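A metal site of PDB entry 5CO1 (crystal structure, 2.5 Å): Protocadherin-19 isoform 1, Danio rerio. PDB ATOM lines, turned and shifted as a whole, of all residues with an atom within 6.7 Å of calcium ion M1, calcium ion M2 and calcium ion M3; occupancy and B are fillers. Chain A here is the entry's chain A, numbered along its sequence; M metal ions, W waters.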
ATOM      1  N   GLU A  15     -14.225 -29.697  -1.162  1.00  0.00           N
ATOM      2  CA  GLU A  15     -13.036 -28.870  -1.238  1.00  0.00           C
ATOM      3  C   GLU A  15     -12.401 -28.836   0.128  1.00  0.00           C
ATOM      4  O   GLU A  15     -13.063 -29.083   1.123  1.00  0.00           O
ATOM      5  CB  GLU A  15     -13.300 -27.471  -1.766  1.00  0.00           C
ATOM      6  CG  GLU A  15     -14.019 -26.521  -0.845  1.00  0.00           C
ATOM      7  CD  GLU A  15     -14.125 -25.142  -1.450  1.00  0.00           C
ATOM      8  OE1 GLU A  15     -13.091 -24.652  -1.983  1.00  0.00           O
ATOM      9  OE2 GLU A  15     -15.245 -24.568  -1.460  1.00  0.00           O
ATOM     10  N   ASN A  16     -11.067 -28.745   0.088  1.00  0.00           N
ATOM     11  CA  ASN A  16     -10.216 -28.626   1.265  1.00  0.00           C
ATOM     12  C   ASN A  16     -10.099 -29.947   1.993  1.00  0.00           C
ATOM     13  O   ASN A  16      -9.652 -30.022   3.129  1.00  0.00           O
ATOM     14  CB  ASN A  16     -10.695 -27.512   2.192  1.00  0.00           C
ATOM     15  CG  ASN A  16     -10.715 -26.137   1.509  1.00  0.00           C
ATOM     16  OD1 ASN A  16      -9.940 -25.854   0.581  1.00  0.00           O
ATOM     17  ND2 ASN A  16     -11.622 -25.272   1.963  1.00  0.00           N
ATOM     18  N   LEU A  70      -7.364 -29.007  -2.687  1.00  0.00           N
ATOM     19  CA  LEU A  70      -8.494 -28.911  -3.601  1.00  0.00           C
ATOM     20  C   LEU A  70      -9.305 -27.672  -3.336  1.00  0.00           C
ATOM     21  O   LEU A  70      -9.977 -27.594  -2.298  1.00  0.00           O
ATOM     22  CB  LEU A  70      -9.416 -30.090  -3.415  1.00  0.00           C
ATOM     23  CG  LEU A  70      -8.959 -31.432  -3.950  1.00  0.00           C
ATOM     24  CD1 LEU A  70     -10.037 -32.439  -3.654  1.00  0.00           C
ATOM     25  CD2 LEU A  70      -8.695 -31.372  -5.444  1.00  0.00           C
ATOM     26  N   ASP A  71      -9.349 -26.758  -4.303  1.00  0.00           N
ATOM     27  CA  ASP A  71     -10.026 -25.471  -4.134  1.00  0.00           C
ATOM     28  C   ASP A  71     -11.053 -25.322  -5.219  1.00  0.00           C
ATOM     29  O   ASP A  71     -10.697 -25.272  -6.395  1.00  0.00           O
ATOM     30  CB  ASP A  71      -9.013 -24.343  -4.184  1.00  0.00           C
ATOM     31  CG  ASP A  71      -9.651 -22.955  -3.977  1.00  0.00           C
ATOM     32  OD1 ASP A  71     -10.851 -22.841  -3.677  1.00  0.00           O
ATOM     33  OD2 ASP A  71      -8.909 -21.970  -4.155  1.00  0.00           O
ATOM     34  N   HIS A  72     -12.333 -25.349  -4.820  1.00  0.00           N
ATOM     35  CA  HIS A  72     -13.438 -25.135  -5.750  1.00  0.00           C
ATOM     36  C   HIS A  72     -13.307 -23.820  -6.529  1.00  0.00           C
ATOM     37  O   HIS A  72     -13.754 -23.711  -7.678  1.00  0.00           O
ATOM     38  CB  HIS A  72     -14.763 -25.118  -4.998  1.00  0.00           C
ATOM     39  CG  HIS A  72     -15.937 -24.767  -5.851  1.00  0.00           C
ATOM     40  ND1 HIS A  72     -16.683 -25.717  -6.501  1.00  0.00           N
ATOM     41  CD2 HIS A  72     -16.502 -23.573  -6.145  1.00  0.00           C
ATOM     42  CE1 HIS A  72     -17.687 -25.130  -7.140  1.00  0.00           C
ATOM     43  NE2 HIS A  72     -17.598 -23.831  -6.936  1.00  0.00           N
ATOM     44  N   GLU A  73     -12.799 -22.794  -5.862  1.00  0.00           N
ATOM     45  CA  GLU A  73     -12.751 -21.458  -6.483  1.00  0.00           C
ATOM     46  C   GLU A  73     -11.632 -21.408  -7.566  1.00  0.00           C
ATOM     47  O   GLU A  73     -11.746 -20.674  -8.550  1.00  0.00           O
ATOM     48  CB  GLU A  73     -12.593 -20.371  -5.416  1.00  0.00           C
ATOM     49  CG  GLU A  73     -13.864 -20.134  -4.601  1.00  0.00           C
ATOM     50  CD  GLU A  73     -14.208 -21.260  -3.600  1.00  0.00           C
ATOM     51  OE1 GLU A  73     -13.304 -21.754  -2.875  1.00  0.00           O
ATOM     52  OE2 GLU A  73     -15.411 -21.636  -3.515  1.00  0.00           O
ATOM     53  N   GLU A  74     -10.656 -22.308  -7.439  1.00  0.00           N
ATOM     54  CA  GLU A  74      -9.621 -22.533  -8.442  1.00  0.00           C
ATOM     55  C   GLU A  74     -10.067 -23.444  -9.592  1.00  0.00           C
ATOM     56  O   GLU A  74      -9.694 -23.210 -10.722  1.00  0.00           O
ATOM     57  CB  GLU A  74      -8.407 -23.119  -7.734  1.00  0.00           C
ATOM     58  CG  GLU A  74      -7.158 -23.292  -8.578  1.00  0.00           C
ATOM     59  CD  GLU A  74      -6.071 -24.095  -7.853  1.00  0.00           C
ATOM     60  OE1 GLU A  74      -4.951 -24.210  -8.377  1.00  0.00           O
ATOM     61  OE2 GLU A  74      -6.355 -24.627  -6.748  1.00  0.00           O
ATOM     62  N   ILE A 103     -16.637 -30.153  -4.410  1.00  0.00           N
ATOM     63  CA  ILE A 103     -17.862 -29.582  -3.921  1.00  0.00           C
ATOM     64  C   ILE A 103     -17.595 -28.363  -3.062  1.00  0.00           C
ATOM     65  O   ILE A 103     -16.686 -28.343  -2.259  1.00  0.00           O
ATOM     66  CB  ILE A 103     -18.740 -30.682  -3.308  1.00  0.00           C
ATOM     67  CG1 ILE A 103     -19.327 -31.432  -4.494  1.00  0.00           C
ATOM     68  CG2 ILE A 103     -19.917 -30.096  -2.521  1.00  0.00           C
ATOM     69  CD1 ILE A 103     -19.534 -32.870  -4.208  1.00  0.00           C
ATOM     70  N   ASP A 104     -18.291 -27.297  -3.392  1.00  0.00           N
ATOM     71  CA  ASP A 104     -18.018 -25.997  -2.800  1.00  0.00           C
ATOM     72  C   ASP A 104     -18.533 -25.966  -1.373  1.00  0.00           C
ATOM     73  O   ASP A 104     -19.624 -26.488  -1.081  1.00  0.00           O
ATOM     74  CB  ASP A 104     -18.668 -24.898  -3.621  1.00  0.00           C
ATOM     75  CG  ASP A 104     -18.733 -23.581  -2.882  1.00  0.00           C
ATOM     76  OD1 ASP A 104     -17.649 -23.036  -2.554  1.00  0.00           O
ATOM     77  OD2 ASP A 104     -19.861 -23.073  -2.674  1.00  0.00           O
ATOM     78  N   ILE A 105     -17.667 -25.501  -0.480  1.00  0.00           N
ATOM     79  CA  ILE A 105     -18.051 -25.038   0.843  1.00  0.00           C
ATOM     80  C   ILE A 105     -17.836 -23.552   1.074  1.00  0.00           C
ATOM     81  O   ILE A 105     -17.161 -22.863   0.292  1.00  0.00           O
ATOM     82  CB  ILE A 105     -17.294 -25.808   1.939  1.00  0.00           C
ATOM     83  CG1 ILE A 105     -15.790 -25.635   1.765  1.00  0.00           C
ATOM     84  CG2 ILE A 105     -17.679 -27.287   1.906  1.00  0.00           C
ATOM     85  CD1 ILE A 105     -15.076 -25.285   3.036  1.00  0.00           C
ATOM     86  N   ASN A 106     -18.473 -23.039   2.126  1.00  0.00           N
ATOM     87  CA  ASN A 106     -18.344 -21.651   2.471  1.00  0.00           C
ATOM     88  C   ASN A 106     -17.015 -21.330   3.161  1.00  0.00           C
ATOM     89  O   ASN A 106     -16.952 -21.138   4.343  1.00  0.00           O
ATOM     90  CB  ASN A 106     -19.476 -21.227   3.348  1.00  0.00           C
ATOM     91  CG  ASN A 106     -19.756 -19.751   3.223  1.00  0.00           C
ATOM     92  OD1 ASN A 106     -19.306 -19.100   2.297  1.00  0.00           O
ATOM     93  ND2 ASN A 106     -20.541 -19.227   4.142  1.00  0.00           N
ATOM     94  N   ASP A 107     -15.958 -21.228   2.393  1.00  0.00           N
ATOM     95  CA  ASP A 107     -14.672 -20.820   2.923  1.00  0.00           C
ATOM     96  C   ASP A 107     -14.290 -19.393   2.474  1.00  0.00           C
ATOM     97  O   ASP A 107     -13.134 -19.051   2.466  1.00  0.00           O
ATOM     98  CB  ASP A 107     -13.595 -21.836   2.506  1.00  0.00           C
ATOM     99  CG  ASP A 107     -13.490 -22.036   0.995  1.00  0.00           C
ATOM    100  OD1 ASP A 107     -14.482 -21.781   0.271  1.00  0.00           O
ATOM    101  OD2 ASP A 107     -12.448 -22.540   0.528  1.00  0.00           O
ATOM    102  N   ASN A 108     -15.262 -18.582   2.065  1.00  0.00           N
ATOM    103  CA  ASN A 108     -14.987 -17.213   1.602  1.00  0.00           C
ATOM    104  C   ASN A 108     -16.002 -16.262   2.142  1.00  0.00           C
ATOM    105  O   ASN A 108     -17.187 -16.387   1.859  1.00  0.00           O
ATOM    106  CB  ASN A 108     -15.011 -17.113   0.074  1.00  0.00           C
ATOM    107  CG  ASN A 108     -13.724 -17.588  -0.577  1.00  0.00           C
ATOM    108  OD1 ASN A 108     -12.723 -16.888  -0.530  1.00  0.00           O
ATOM    109  ND2 ASN A 108     -13.718 -18.829  -1.086  1.00  0.00           N
ATOM    110  N   ALA A 109     -15.520 -15.282   2.885  1.00  0.00           N
ATOM    111  CA  ALA A 109     -16.335 -14.213   3.449  1.00  0.00           C
ATOM    112  C   ALA A 109     -16.707 -13.225   2.361  1.00  0.00           C
ATOM    113  O   ALA A 109     -16.060 -13.165   1.311  1.00  0.00           O
ATOM    114  CB  ALA A 109     -15.552 -13.503   4.541  1.00  0.00           C
ATOM    115  N   PRO A 110     -17.742 -12.413   2.610  1.00  0.00           N
ATOM    116  CA  PRO A 110     -18.108 -11.411   1.616  1.00  0.00           C
ATOM    117  C   PRO A 110     -17.114 -10.274   1.559  1.00  0.00           C
ATOM    118  O   PRO A 110     -16.629  -9.871   2.607  1.00  0.00           O
ATOM    119  CB  PRO A 110     -19.469 -10.909   2.089  1.00  0.00           C
ATOM    120  CG  PRO A 110     -20.022 -11.989   2.929  1.00  0.00           C
ATOM    121  CD  PRO A 110     -18.849 -12.695   3.540  1.00  0.00           C
ATOM    122  N   ASP A 141     -18.857 -12.396  -3.222  1.00  0.00           N
ATOM    123  CA  ASP A 141     -18.418 -13.568  -2.530  1.00  0.00           C
ATOM    124  C   ASP A 141     -17.934 -14.540  -3.604  1.00  0.00           C
ATOM    125  O   ASP A 141     -18.683 -14.911  -4.506  1.00  0.00           O
ATOM    126  CB  ASP A 141     -19.607 -14.172  -1.742  1.00  0.00           C
ATOM    127  CG  ASP A 141     -19.179 -15.082  -0.582  1.00  0.00           C
ATOM    128  OD1 ASP A 141     -18.520 -16.106  -0.839  1.00  0.00           O
ATOM    129  OD2 ASP A 141     -19.580 -14.827   0.572  1.00  0.00           O
ATOM    130  N   ASN A 142     -16.696 -14.980  -3.475  1.00  0.00           N
ATOM    131  CA  ASN A 142     -16.143 -15.972  -4.375  1.00  0.00           C
ATOM    132  C   ASN A 142     -16.768 -17.369  -4.327  1.00  0.00           C
ATOM    133  O   ASN A 142     -16.398 -18.202  -5.129  1.00  0.00           O
ATOM    134  CB  ASN A 142     -14.628 -16.124  -4.158  1.00  0.00           C
ATOM    135  CG  ASN A 142     -13.895 -14.795  -4.255  1.00  0.00           C
ATOM    136  OD1 ASN A 142     -14.101 -14.031  -5.183  1.00  0.00           O
ATOM    137  ND2 ASN A 142     -13.088 -14.501  -3.248  1.00  0.00           N
ATOM    138  N   ASP A 143     -17.614 -17.670  -3.333  1.00  0.00           N
ATOM    139  CA  ASP A 143     -18.224 -19.016  -3.234  1.00  0.00           C
ATOM    140  C   ASP A 143     -19.404 -19.094  -4.207  1.00  0.00           C
ATOM    141  O   ASP A 143     -19.831 -18.069  -4.734  1.00  0.00           O
ATOM    142  CB  ASP A 143     -18.692 -19.343  -1.788  1.00  0.00           C
ATOM    143  CG  ASP A 143     -17.556 -19.339  -0.767  1.00  0.00           C
ATOM    144  OD1 ASP A 143     -16.533 -20.045  -1.003  1.00  0.00           O
ATOM    145  OD2 ASP A 143     -17.697 -18.643   0.276  1.00  0.00           O
ATOM    146  N   SER A 144     -19.956 -20.294  -4.398  1.00  0.00           N
ATOM    147  CA  SER A 144     -21.139 -20.483  -5.244  1.00  0.00           C
ATOM    148  C   SER A 144     -22.419 -20.771  -4.470  1.00  0.00           C
ATOM    149  O   SER A 144     -22.422 -20.881  -3.259  1.00  0.00           O
ATOM    150  CB  SER A 144     -20.876 -21.624  -6.231  1.00  0.00           C
ATOM    151  OG  SER A 144     -19.620 -21.418  -6.872  1.00  0.00           O
ATOM    152  N   ALA A 146     -25.796 -20.534  -2.406  1.00  0.00           N
ATOM    153  CA  ALA A 146     -26.121 -19.813  -1.185  1.00  0.00           C
ATOM    154  C   ALA A 146     -24.866 -19.285  -0.510  1.00  0.00           C
ATOM    155  O   ALA A 146     -24.907 -18.232   0.124  1.00  0.00           O
ATOM    156  CB  ALA A 146     -26.852 -20.743  -0.221  1.00  0.00           C
ATOM    157  N   ASN A 147     -23.785 -20.049  -0.604  1.00  0.00           N
ATOM    158  CA  ASN A 147     -22.537 -19.667   0.058  1.00  0.00           C
ATOM    159  C   ASN A 147     -22.039 -18.355  -0.466  1.00  0.00           C
ATOM    160  O   ASN A 147     -21.155 -17.740   0.150  1.00  0.00           O
ATOM    161  CB  ASN A 147     -21.473 -20.676  -0.223  1.00  0.00           C
ATOM    162  CG  ASN A 147     -21.737 -21.999   0.442  1.00  0.00           C
ATOM    163  OD1 ASN A 147     -22.285 -22.057   1.536  1.00  0.00           O
ATOM    164  ND2 ASN A 147     -21.129 -23.051  -0.109  1.00  0.00           N
ATOM    165  N   GLY A 148     -22.435 -18.065  -1.700  1.00  0.00           N
ATOM    166  CA  GLY A 148     -22.053 -16.839  -2.381  1.00  0.00           C
ATOM    167  C   GLY A 148     -23.078 -15.712  -2.470  1.00  0.00           C
ATOM    168  O   GLY A 148     -22.708 -14.631  -2.895  1.00  0.00           O
ATOM    169  N   LYS A 149     -24.364 -15.979  -2.160  1.00  0.00           N
ATOM    170  CA  LYS A 149     -25.413 -14.947  -2.036  1.00  0.00           C
ATOM    171  C   LYS A 149     -25.227 -14.114  -0.775  1.00  0.00           C
ATOM    172  O   LYS A 149     -25.381 -14.623   0.318  1.00  0.00           O
ATOM    173  CB  LYS A 149     -26.822 -15.551  -1.948  1.00  0.00           C
ATOM    174  CG  LYS A 149     -27.369 -16.121  -3.254  1.00  0.00           C
ATOM    175  CD  LYS A 149     -28.448 -15.220  -3.882  1.00  0.00           C
ATOM    176  CE  LYS A 149     -28.392 -15.250  -5.411  1.00  0.00           C
ATOM    177  NZ  LYS A 149     -28.159 -16.622  -5.974  1.00  0.00           N
ATOM    178  N   VAL A 150     -25.183 -12.805  -0.952  1.00  0.00           N
ATOM    179  CA  VAL A 150     -24.781 -11.889   0.089  1.00  0.00           C
ATOM    180  C   VAL A 150     -25.863 -10.857   0.336  1.00  0.00           C
ATOM    181  O   VAL A 150     -26.706 -10.642  -0.493  1.00  0.00           O
ATOM    182  CB  VAL A 150     -23.519 -11.146  -0.354  1.00  0.00           C
ATOM    183  CG1 VAL A 150     -23.182 -10.005   0.593  1.00  0.00           C
ATOM    184  CG2 VAL A 150     -22.383 -12.142  -0.428  1.00  0.00           C
ATOM    185  N   ASP A 193     -23.303 -13.586   4.120  1.00  0.00           N
ATOM    186  CA  ASP A 193     -23.633 -14.534   3.095  1.00  0.00           C
ATOM    187  C   ASP A 193     -24.576 -15.545   3.661  1.00  0.00           C
ATOM    188  O   ASP A 193     -24.949 -15.434   4.808  1.00  0.00           O
ATOM    189  CB  ASP A 193     -22.369 -15.181   2.533  1.00  0.00           C
ATOM    190  CG  ASP A 193     -21.769 -16.204   3.468  1.00  0.00           C
ATOM    191  OD1 ASP A 193     -22.552 -16.846   4.208  1.00  0.00           O
ATOM    192  OD2 ASP A 193     -20.525 -16.403   3.381  1.00  0.00           O
ATOM    193  N   SER A 194     -25.069 -16.461   2.849  1.00  0.00           N
ATOM    194  CA  SER A 194     -26.196 -17.292   3.244  1.00  0.00           C
ATOM    195  C   SER A 194     -25.802 -18.757   3.282  1.00  0.00           C
ATOM    196  O   SER A 194     -26.645 -19.649   3.188  1.00  0.00           O
ATOM    197  CB  SER A 194     -27.340 -17.075   2.272  1.00  0.00           C
ATOM    198  OG  SER A 194     -27.524 -15.686   2.102  1.00  0.00           O
ATOM    199  N   GLY A 195     -24.502 -18.995   3.352  1.00  0.00           N
ATOM    200  CA  GLY A 195     -23.961 -20.315   3.566  1.00  0.00           C
ATOM    201  C   GLY A 195     -24.115 -20.737   5.008  1.00  0.00           C
ATOM    202  O   GLY A 195     -24.715 -20.029   5.815  1.00  0.00           O
ATOM    203  N   LEU A 199     -20.817 -16.618   6.986  1.00  0.00           N
ATOM    204  CA  LEU A 199     -19.652 -15.811   7.216  1.00  0.00           C
ATOM    205  C   LEU A 199     -20.010 -14.353   6.982  1.00  0.00           C
ATOM    206  O   LEU A 199     -20.912 -14.019   6.206  1.00  0.00           O
ATOM    207  CB  LEU A 199     -18.541 -16.193   6.242  1.00  0.00           C
ATOM    208  CG  LEU A 199     -17.837 -17.536   6.414  1.00  0.00           C
ATOM    209  CD1 LEU A 199     -16.944 -17.796   5.208  1.00  0.00           C
ATOM    210  CD2 LEU A 199     -17.024 -17.584   7.686  1.00  0.00           C
HETATM  211 CA    CA M   1     -15.829 -22.365  -1.414  1.00  0.00          CA
HETATM  212 CA    CA M   2     -11.880 -22.571  -1.538  1.00  0.00          CA
HETATM  213 CA    CA M   3     -19.220 -17.096   1.228  1.00  0.00          CA
HETATM  214  O   HOH W   1      -9.880 -23.550  -1.112  1.00  0.00           O
HETATM  215  O   HOH W   2     -11.042 -20.327  -1.419  1.00  0.00           O
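Within 4 Å of calcium ion M1: Glu 15, Glu 73, Asp 104, Ile 105, Asp 107 and Asp 143.
The nearest printed residue that does not touch calcium ion M1 is Asn 108 (4.1 Å).
Calcium ion M3 is bound by O of Asn 108, at 2.2 Å.
The side-chain amide oxygen (OD1) of Asn 106 binds calcium ion M3 (2.3 Å).
O of Asn 147 binds calcium ion M3, at 2.3 Å.
OD2 of Asp 143 binds calcium ion M3 (2.4 Å).
Calcium ion M3 is bound by OD2 of Asp 141 (2.4 Å).
The side-chain carboxylate (OD1) of Asp 141 binds calcium ion M3 (2.4 Å).
OD2 of Asp 193 is bound to calcium ion M3 (2.6 Å).
Calcium ion M3 has seven donor atoms within binding distance.
Of the 28 residues printed, 4 come within 4 Å of calcium ion M2.
The nearest printed residue that does not touch calcium ion M2 is Asn 108 (4.2 Å).
Calcium ion M2 is bound by OE1 of Glu 73 (2.1 Å), OD2 of Asp 107 (2.1 Å), water W1 (2.3 Å), OD1 of Asp 71 (2.4 Å), water W2 (2.4 Å) and OE1 of Glu 15 (2.4 Å).
Calcium ion M2 has six donor atoms within binding distance.
The backbone NH (N) of Ser 144 is in hydrogen-bond range of the side-chain carboxylate (OD2) of Asp 104, 3.3 Å away.
The backbone carbonyl oxygen of Leu 199 lies within hydrogen-bond range of the backbone NH of Asp 193 (3.2 Å).
OE1 of Glu 73 sits close to ND2 of Asn 108, at 3.5 Å.
OD1 of Asp 193 is in hydrogen-bond range of N of Gly 195, 3.0 Å away.
N of Glu 15 is in hydrogen-bond range of O of Ile 103 (3.0 Å).
OE1 of Glu 15 sits close to N of His 72 (3.0 Å).
OD1 of Asp 107 lies close to ND2 of Asn 108, 3.3 Å away.
The side-chain amide nitrogen of Asn 147 sits at hydrogen-bond distance from the side-chain carboxylate of Asp 104.
Calcium ion M1 is bound by O of Ile 105, OD1 of Asp 107, OD1 of Asp 104, OE2 of Glu 73, OE2 of Glu 15 and OD1 of Asp 143.
Calcium ion M1 has six donor atoms within binding distance.
Slightly farther from calcium ion M1 lies OE1 of Glu 73 (3.0 Å).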
